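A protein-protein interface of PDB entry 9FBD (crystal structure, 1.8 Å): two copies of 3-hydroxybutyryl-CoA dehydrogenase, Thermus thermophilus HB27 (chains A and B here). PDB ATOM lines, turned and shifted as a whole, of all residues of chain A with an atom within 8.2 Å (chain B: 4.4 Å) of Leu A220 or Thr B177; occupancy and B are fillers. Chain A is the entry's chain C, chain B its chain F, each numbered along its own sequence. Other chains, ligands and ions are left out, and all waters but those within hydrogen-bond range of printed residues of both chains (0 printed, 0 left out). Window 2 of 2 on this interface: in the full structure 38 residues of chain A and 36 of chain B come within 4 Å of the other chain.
Of the printed residues of chain B, Ala A213 touches Leu B179. Printed residues of chain B within 4 Å of Gly A216: Leu B179. Of the printed residues of chain B, Ile A217 touches Leu B150 and Leu B179. Printed residues of chain B within 4 Å of Leu A220: Met B148 and Thr B177. Printed residues of chain B within 4 Å of Gly A221: Met B148 (3.1 Å) and Leu B150 (3.5 Å). Printed residues of chain A within 4 Å of Met B148: Leu A220, Gly A221 and Asn A223. Of chain A, only Leu A220 (3.8 Å) comes within 4 Å of Thr B177. No residue of chain A comes within 4 Å of Pro B178. The nearest residue of chain A that does not touch Thr B177 is Gly A216 (6.8 Å).
Hydrophobic or aromatic side chains of chain B that line the printed part of chain A: Met B148, Leu B150 and Leu B179. Hydrophobic or aromatic side chains of chain A within 4 Å of the printed part of chain B: Ile A217 and Leu A220.
The backbone carbonyl oxygen (O) of Val B151 lies within hydrogen-bond range of the backbone NH (N) of Leu B179 (2.9 Å). O of Met A218 is in hydrogen-bond range of N of Asn A223, 3.4 Å away. N of Val B151 sits at hydrogen-bond distance from O of Thr B177, 3.1 Å away. N of Thr B177 is in hydrogen-bond range of O of Gln B149, 2.7 Å away. The backbone carbonyl oxygen of Met B148 lies within hydrogen-bond range of the side-chain amino group of Lys B176.
O of Ala A213 touches CD1 of Leu B179 (3.7 Å). Leu B179 touches Gly A216. CD2 of Leu B150 touches O of Ile A217, at 3.5 Å. Ile A217 touches Leu B179. Met B148 touches Leu A220. Thr B177 touches Leu A220 (CB to CD1, 3.8 Å). O of Gly A221 touches CE of Met B148 (3.1 Å). Gly A221 touches Leu B150. Asn A223 touches Met B148 (ND2 to CE, 3.99 Å).
No position is printed for both chains. Of the 9 pairs that touch across the chains among the printed residues, none has its exchanged pair printed and touching as well.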
ATOM      1  N   GLU A 212      -4.577   7.687  35.290  1.00  0.00           N
ATOM      2  CA  GLU A 212      -5.004   7.258  33.930  1.00  0.00           C
ATOM      3  C   GLU A 212      -6.505   7.522  33.778  1.00  0.00           C
ATOM      4  O   GLU A 212      -6.928   8.030  32.736  1.00  0.00           O
ATOM      5  CB  GLU A 212      -4.698   5.771  33.693  1.00  0.00           C
ATOM      6  CG  GLU A 212      -3.216   5.458  33.639  1.00  0.00           C
ATOM      7  CD  GLU A 212      -2.514   5.219  34.976  1.00  0.00           C
ATOM      8  OE1 GLU A 212      -3.194   5.111  36.033  1.00  0.00           O
ATOM      9  OE2 GLU A 212      -1.273   5.150  34.960  1.00  0.00           O
ATOM     10  N   ALA A 213      -7.294   7.191  34.793  1.00  0.00           N
ATOM     11  CA  ALA A 213      -8.761   7.351  34.745  1.00  0.00           C
ATOM     12  C   ALA A 213      -9.076   8.843  34.673  1.00  0.00           C
ATOM     13  O   ALA A 213      -9.879   9.247  33.825  1.00  0.00           O
ATOM     14  CB  ALA A 213      -9.393   6.663  35.916  1.00  0.00           C
ATOM     15  N   ILE A 214      -8.402   9.650  35.485  1.00  0.00           N
ATOM     16  CA  ILE A 214      -8.648  11.117  35.531  1.00  0.00           C
ATOM     17  C   ILE A 214      -8.308  11.716  34.163  1.00  0.00           C
ATOM     18  O   ILE A 214      -9.148  12.446  33.613  1.00  0.00           O
ATOM     19  CB  ILE A 214      -7.863  11.777  36.671  1.00  0.00           C
ATOM     20  CG1 ILE A 214      -8.418  11.352  38.025  1.00  0.00           C
ATOM     21  CG2 ILE A 214      -7.850  13.282  36.501  1.00  0.00           C
ATOM     22  CD1 ILE A 214      -7.515  11.681  39.199  1.00  0.00           C
ATOM     23  N   ASP A 215      -7.133  11.423  33.621  1.00  0.00           N
ATOM     24  CA  ASP A 215      -6.724  12.019  32.322  1.00  0.00           C
ATOM     25  C   ASP A 215      -7.618  11.496  31.187  1.00  0.00           C
ATOM     26  O   ASP A 215      -7.992  12.283  30.307  1.00  0.00           O
ATOM     27  CB  ASP A 215      -5.222  11.812  32.087  1.00  0.00           C
ATOM     28  CG  ASP A 215      -4.367  12.780  32.887  1.00  0.00           C
ATOM     29  OD1 ASP A 215      -4.924  13.778  33.412  1.00  0.00           O
ATOM     30  OD2 ASP A 215      -3.147  12.526  32.993  1.00  0.00           O
ATOM     31  N   GLY A 216      -7.961  10.212  31.214  1.00  0.00           N
ATOM     32  CA  GLY A 216      -8.819   9.576  30.191  1.00  0.00           C
ATOM     33  C   GLY A 216     -10.213  10.178  30.191  1.00  0.00           C
ATOM     34  O   GLY A 216     -10.770  10.432  29.092  1.00  0.00           O
ATOM     35  N   ILE A 217     -10.765  10.424  31.379  1.00  0.00           N
ATOM     36  CA  ILE A 217     -12.119  11.016  31.509  1.00  0.00           C
ATOM     37  C   ILE A 217     -12.100  12.404  30.866  1.00  0.00           C
ATOM     38  O   ILE A 217     -13.039  12.713  30.111  1.00  0.00           O
ATOM     39  CB  ILE A 217     -12.595  11.014  32.973  1.00  0.00           C
ATOM     40  CG1 ILE A 217     -12.971   9.602  33.404  1.00  0.00           C
ATOM     41  CG2 ILE A 217     -13.733  12.017  33.179  1.00  0.00           C
ATOM     42  CD1 ILE A 217     -13.063   9.430  34.902  1.00  0.00           C
ATOM     43  N   MET A 218     -11.074  13.210  31.116  1.00  0.00           N
ATOM     44  CA  MET A 218     -11.071  14.595  30.591  1.00  0.00           C
ATOM     45  C   MET A 218     -10.775  14.578  29.078  1.00  0.00           C
ATOM     46  O   MET A 218     -11.373  15.402  28.343  1.00  0.00           O
ATOM     47  CB  MET A 218     -10.077  15.476  31.350  1.00  0.00           C
ATOM     48  CG  MET A 218     -10.412  15.585  32.836  1.00  0.00           C
ATOM     49  SD  MET A 218     -12.150  16.025  33.143  1.00  0.00           S
ATOM     50  CE  MET A 218     -12.127  17.715  32.549  1.00  0.00           C
ATOM     51  N   ARG A 219      -9.915  13.680  28.602  1.00  0.00           N
ATOM     52  CA  ARG A 219      -9.623  13.570  27.141  1.00  0.00           C
ATOM     53  C   ARG A 219     -10.880  13.095  26.395  1.00  0.00           C
ATOM     54  O   ARG A 219     -11.312  13.765  25.445  1.00  0.00           O
ATOM     55  CB  ARG A 219      -8.520  12.544  26.853  1.00  0.00           C
ATOM     56  CG  ARG A 219      -7.106  13.088  26.848  1.00  0.00           C
ATOM     57  CD  ARG A 219      -6.154  12.025  26.308  1.00  0.00           C
ATOM     58  NE  ARG A 219      -5.287  11.578  27.377  1.00  0.00           N
ATOM     59  CZ  ARG A 219      -5.340  10.415  28.026  1.00  0.00           C
ATOM     60  NH1 ARG A 219      -4.469  10.196  28.993  1.00  0.00           N
ATOM     61  NH2 ARG A 219      -6.209   9.471  27.707  1.00  0.00           N
ATOM     62  N   LEU A 220     -11.441  11.960  26.804  1.00  0.00           N
ATOM     63  CA  LEU A 220     -12.515  11.274  26.050  1.00  0.00           C
ATOM     64  C   LEU A 220     -13.855  11.963  26.322  1.00  0.00           C
ATOM     65  O   LEU A 220     -14.646  12.084  25.384  1.00  0.00           O
ATOM     66  CB  LEU A 220     -12.561   9.802  26.443  1.00  0.00           C
ATOM     67  CG  LEU A 220     -11.342   8.970  26.041  1.00  0.00           C
ATOM     68  CD1 LEU A 220     -11.510   7.532  26.518  1.00  0.00           C
ATOM     69  CD2 LEU A 220     -11.094   9.019  24.532  1.00  0.00           C
ATOM     70  N   GLY A 221     -14.109  12.390  27.559  1.00  0.00           N
ATOM     71  CA  GLY A 221     -15.418  12.942  27.952  1.00  0.00           C
ATOM     72  C   GLY A 221     -15.547  14.396  27.550  1.00  0.00           C
ATOM     73  O   GLY A 221     -16.617  14.784  27.082  1.00  0.00           O
ATOM     74  N   MET A 222     -14.491  15.180  27.729  1.00  0.00           N
ATOM     75  CA  MET A 222     -14.558  16.652  27.580  1.00  0.00           C
ATOM     76  C   MET A 222     -13.795  17.073  26.327  1.00  0.00           C
ATOM     77  O   MET A 222     -13.799  18.284  26.034  1.00  0.00           O
ATOM     78  CB  MET A 222     -13.986  17.334  28.833  1.00  0.00           C
ATOM     79  CG  MET A 222     -15.028  17.732  29.875  1.00  0.00           C
ATOM     80  SD  MET A 222     -16.321  16.521  30.288  1.00  0.00           S
ATOM     81  CE  MET A 222     -15.436  15.342  31.315  1.00  0.00           C
ATOM     82  N   ASN A 223     -13.169  16.136  25.609  1.00  0.00           N
ATOM     83  CA  ASN A 223     -12.360  16.443  24.396  1.00  0.00           C
ATOM     84  C   ASN A 223     -11.252  17.455  24.700  1.00  0.00           C
ATOM     85  O   ASN A 223     -10.946  18.258  23.816  1.00  0.00           O
ATOM     86  CB  ASN A 223     -13.247  16.947  23.259  1.00  0.00           C
ATOM     87  CG  ASN A 223     -13.963  15.795  22.597  1.00  0.00           C
ATOM     88  OD1 ASN A 223     -13.318  14.930  22.009  1.00  0.00           O
ATOM     89  ND2 ASN A 223     -15.279  15.740  22.728  1.00  0.00           N
ATOM     90  N   HIS A 224     -10.660  17.425  25.896  1.00  0.00           N
ATOM     91  CA  HIS A 224      -9.395  18.153  26.172  1.00  0.00           C
ATOM     92  C   HIS A 224      -8.289  17.362  25.482  1.00  0.00           C
ATOM     93  O   HIS A 224      -8.280  16.136  25.588  1.00  0.00           O
ATOM     94  CB  HIS A 224      -9.138  18.306  27.678  1.00  0.00           C
ATOM     95  CG  HIS A 224     -10.119  19.166  28.399  1.00  0.00           C
ATOM     96  ND1 HIS A 224     -11.127  19.870  27.753  1.00  0.00           N
ATOM     97  CD2 HIS A 224     -10.223  19.467  29.710  1.00  0.00           C
ATOM     98  CE1 HIS A 224     -11.828  20.539  28.646  1.00  0.00           C
ATOM     99  NE2 HIS A 224     -11.297  20.301  29.865  1.00  0.00           N
ATOM    100  N   PRO A 225      -7.357  18.003  24.742  1.00  0.00           N
ATOM    101  CA  PRO A 225      -6.306  17.267  24.036  1.00  0.00           C
ATOM    102  C   PRO A 225      -5.379  16.535  25.021  1.00  0.00           C
ATOM    103  O   PRO A 225      -4.979  15.443  24.731  1.00  0.00           O
ATOM    104  CB  PRO A 225      -5.521  18.330  23.256  1.00  0.00           C
ATOM    105  CG  PRO A 225      -6.395  19.575  23.286  1.00  0.00           C
ATOM    106  CD  PRO A 225      -7.296  19.448  24.501  1.00  0.00           C
ATOM    107  N   MET A 226      -5.117  17.134  26.185  1.00  0.00           N
ATOM    108  CA  MET A 226      -4.375  16.479  27.288  1.00  0.00           C
ATOM    109  C   MET A 226      -5.231  16.497  28.555  1.00  0.00           C
ATOM    110  O   MET A 226      -5.855  17.533  28.841  1.00  0.00           O
ATOM    111  CB  MET A 226      -3.060  17.217  27.558  1.00  0.00           C
ATOM    112  CG  MET A 226      -1.938  16.842  26.614  1.00  0.00           C
ATOM    113  SD  MET A 226      -0.400  17.596  27.207  1.00  0.00           S
ATOM    114  CE  MET A 226       0.278  16.245  28.150  1.00  0.00           C
ATOM    115  N   GLY A 227      -5.198  15.410  29.311  1.00  0.00           N
ATOM    116  CA  GLY A 227      -5.759  15.370  30.663  1.00  0.00           C
ATOM    117  C   GLY A 227      -4.983  16.290  31.594  1.00  0.00           C
ATOM    118  O   GLY A 227      -3.840  16.643  31.319  1.00  0.00           O
ATOM    119  N   MET B 148     -19.784   9.249  21.903  1.00  0.00           N
ATOM    120  CA  MET B 148     -18.821   9.488  23.017  1.00  0.00           C
ATOM    121  C   MET B 148     -18.344   8.143  23.565  1.00  0.00           C
ATOM    122  O   MET B 148     -19.179   7.333  24.044  1.00  0.00           O
ATOM    123  CB  MET B 148     -19.456  10.314  24.134  1.00  0.00           C
ATOM    124  CG  MET B 148     -19.880  11.700  23.664  1.00  0.00           C
ATOM    125  SD  MET B 148     -18.506  12.716  23.056  1.00  0.00           S
ATOM    126  CE  MET B 148     -17.734  13.208  24.597  1.00  0.00           C
ATOM    127  N   GLN B 149     -17.028   7.914  23.497  1.00  0.00           N
ATOM    128  CA  GLN B 149     -16.403   6.612  23.848  1.00  0.00           C
ATOM    129  C   GLN B 149     -16.399   6.403  25.356  1.00  0.00           C
ATOM    130  O   GLN B 149     -16.329   5.245  25.769  1.00  0.00           O
ATOM    131  CB  GLN B 149     -14.985   6.532  23.297  1.00  0.00           C
ATOM    132  CG  GLN B 149     -14.935   5.894  21.921  1.00  0.00           C
ATOM    133  CD  GLN B 149     -13.955   6.547  20.978  1.00  0.00           C
ATOM    134  OE1 GLN B 149     -13.027   7.254  21.376  1.00  0.00           O
ATOM    135  NE2 GLN B 149     -14.191   6.317  19.703  1.00  0.00           N
ATOM    136  N   LEU B 150     -16.482   7.465  26.154  1.00  0.00           N
ATOM    137  CA  LEU B 150     -16.334   7.359  27.623  1.00  0.00           C
ATOM    138  C   LEU B 150     -17.588   6.781  28.285  1.00  0.00           C
ATOM    139  O   LEU B 150     -18.700   7.254  28.008  1.00  0.00           O
ATOM    140  CB  LEU B 150     -16.027   8.744  28.183  1.00  0.00           C
ATOM    141  CG  LEU B 150     -15.768   8.763  29.687  1.00  0.00           C
ATOM    142  CD1 LEU B 150     -14.615   7.844  30.068  1.00  0.00           C
ATOM    143  CD2 LEU B 150     -15.496  10.184  30.153  1.00  0.00           C
ATOM    144  N   VAL B 151     -17.383   5.841  29.205  1.00  0.00           N
ATOM    145  CA  VAL B 151     -18.335   5.550  30.308  1.00  0.00           C
ATOM    146  C   VAL B 151     -17.587   5.739  31.629  1.00  0.00           C
ATOM    147  O   VAL B 151     -16.553   5.089  31.845  1.00  0.00           O
ATOM    148  CB  VAL B 151     -18.956   4.145  30.218  1.00  0.00           C
ATOM    149  CG1 VAL B 151     -19.946   3.934  31.342  1.00  0.00           C
ATOM    150  CG2 VAL B 151     -19.622   3.898  28.881  1.00  0.00           C
ATOM    151  N   LYS B 176     -17.040   1.061  24.151  1.00  0.00           N
ATOM    152  CA  LYS B 176     -16.745   2.223  25.029  1.00  0.00           C
ATOM    153  C   LYS B 176     -15.465   1.955  25.818  1.00  0.00           C
ATOM    154  O   LYS B 176     -15.066   0.775  25.952  1.00  0.00           O
ATOM    155  CB  LYS B 176     -17.882   2.475  26.023  1.00  0.00           C
ATOM    156  CG  LYS B 176     -19.251   2.750  25.423  1.00  0.00           C
ATOM    157  CD  LYS B 176     -19.232   3.850  24.401  1.00  0.00           C
ATOM    158  CE  LYS B 176     -20.597   4.414  24.109  1.00  0.00           C
ATOM    159  NZ  LYS B 176     -20.544   5.138  22.823  1.00  0.00           N
ATOM    160  N   THR B 177     -14.883   3.012  26.373  1.00  0.00           N
ATOM    161  CA  THR B 177     -13.782   2.937  27.355  1.00  0.00           C
ATOM    162  C   THR B 177     -14.367   3.230  28.730  1.00  0.00           C
ATOM    163  O   THR B 177     -14.677   4.383  29.041  1.00  0.00           O
ATOM    164  CB  THR B 177     -12.681   3.929  26.985  1.00  0.00           C
ATOM    165  OG1 THR B 177     -12.436   3.755  25.589  1.00  0.00           O
ATOM    166  CG2 THR B 177     -11.438   3.748  27.831  1.00  0.00           C
ATOM    167  N   PRO B 178     -14.550   2.196  29.573  1.00  0.00           N
ATOM    168  CA  PRO B 178     -15.028   2.387  30.938  1.00  0.00           C
ATOM    169  C   PRO B 178     -13.870   2.827  31.841  1.00  0.00           C
ATOM    170  O   PRO B 178     -12.856   2.176  31.865  1.00  0.00           O
ATOM    171  CB  PRO B 178     -15.515   0.997  31.351  1.00  0.00           C
ATOM    172  CG  PRO B 178     -14.613   0.044  30.557  1.00  0.00           C
ATOM    173  CD  PRO B 178     -14.288   0.777  29.263  1.00  0.00           C
ATOM    174  N   LEU B 179     -14.038   3.943  32.544  1.00  0.00           N
ATOM    175  CA  LEU B 179     -13.030   4.428  33.508  1.00  0.00           C
ATOM    176  C   LEU B 179     -13.724   4.548  34.854  1.00  0.00           C
ATOM    177  O   LEU B 179     -14.836   5.125  34.948  1.00  0.00           O
ATOM    178  CB  LEU B 179     -12.420   5.733  32.995  1.00  0.00           C
ATOM    179  CG  LEU B 179     -11.615   5.590  31.694  1.00  0.00           C
ATOM    180  CD1 LEU B 179     -11.137   6.939  31.190  1.00  0.00           C
ATOM    181  CD2 LEU B 179     -10.416   4.645  31.851  1.00  0.00           C
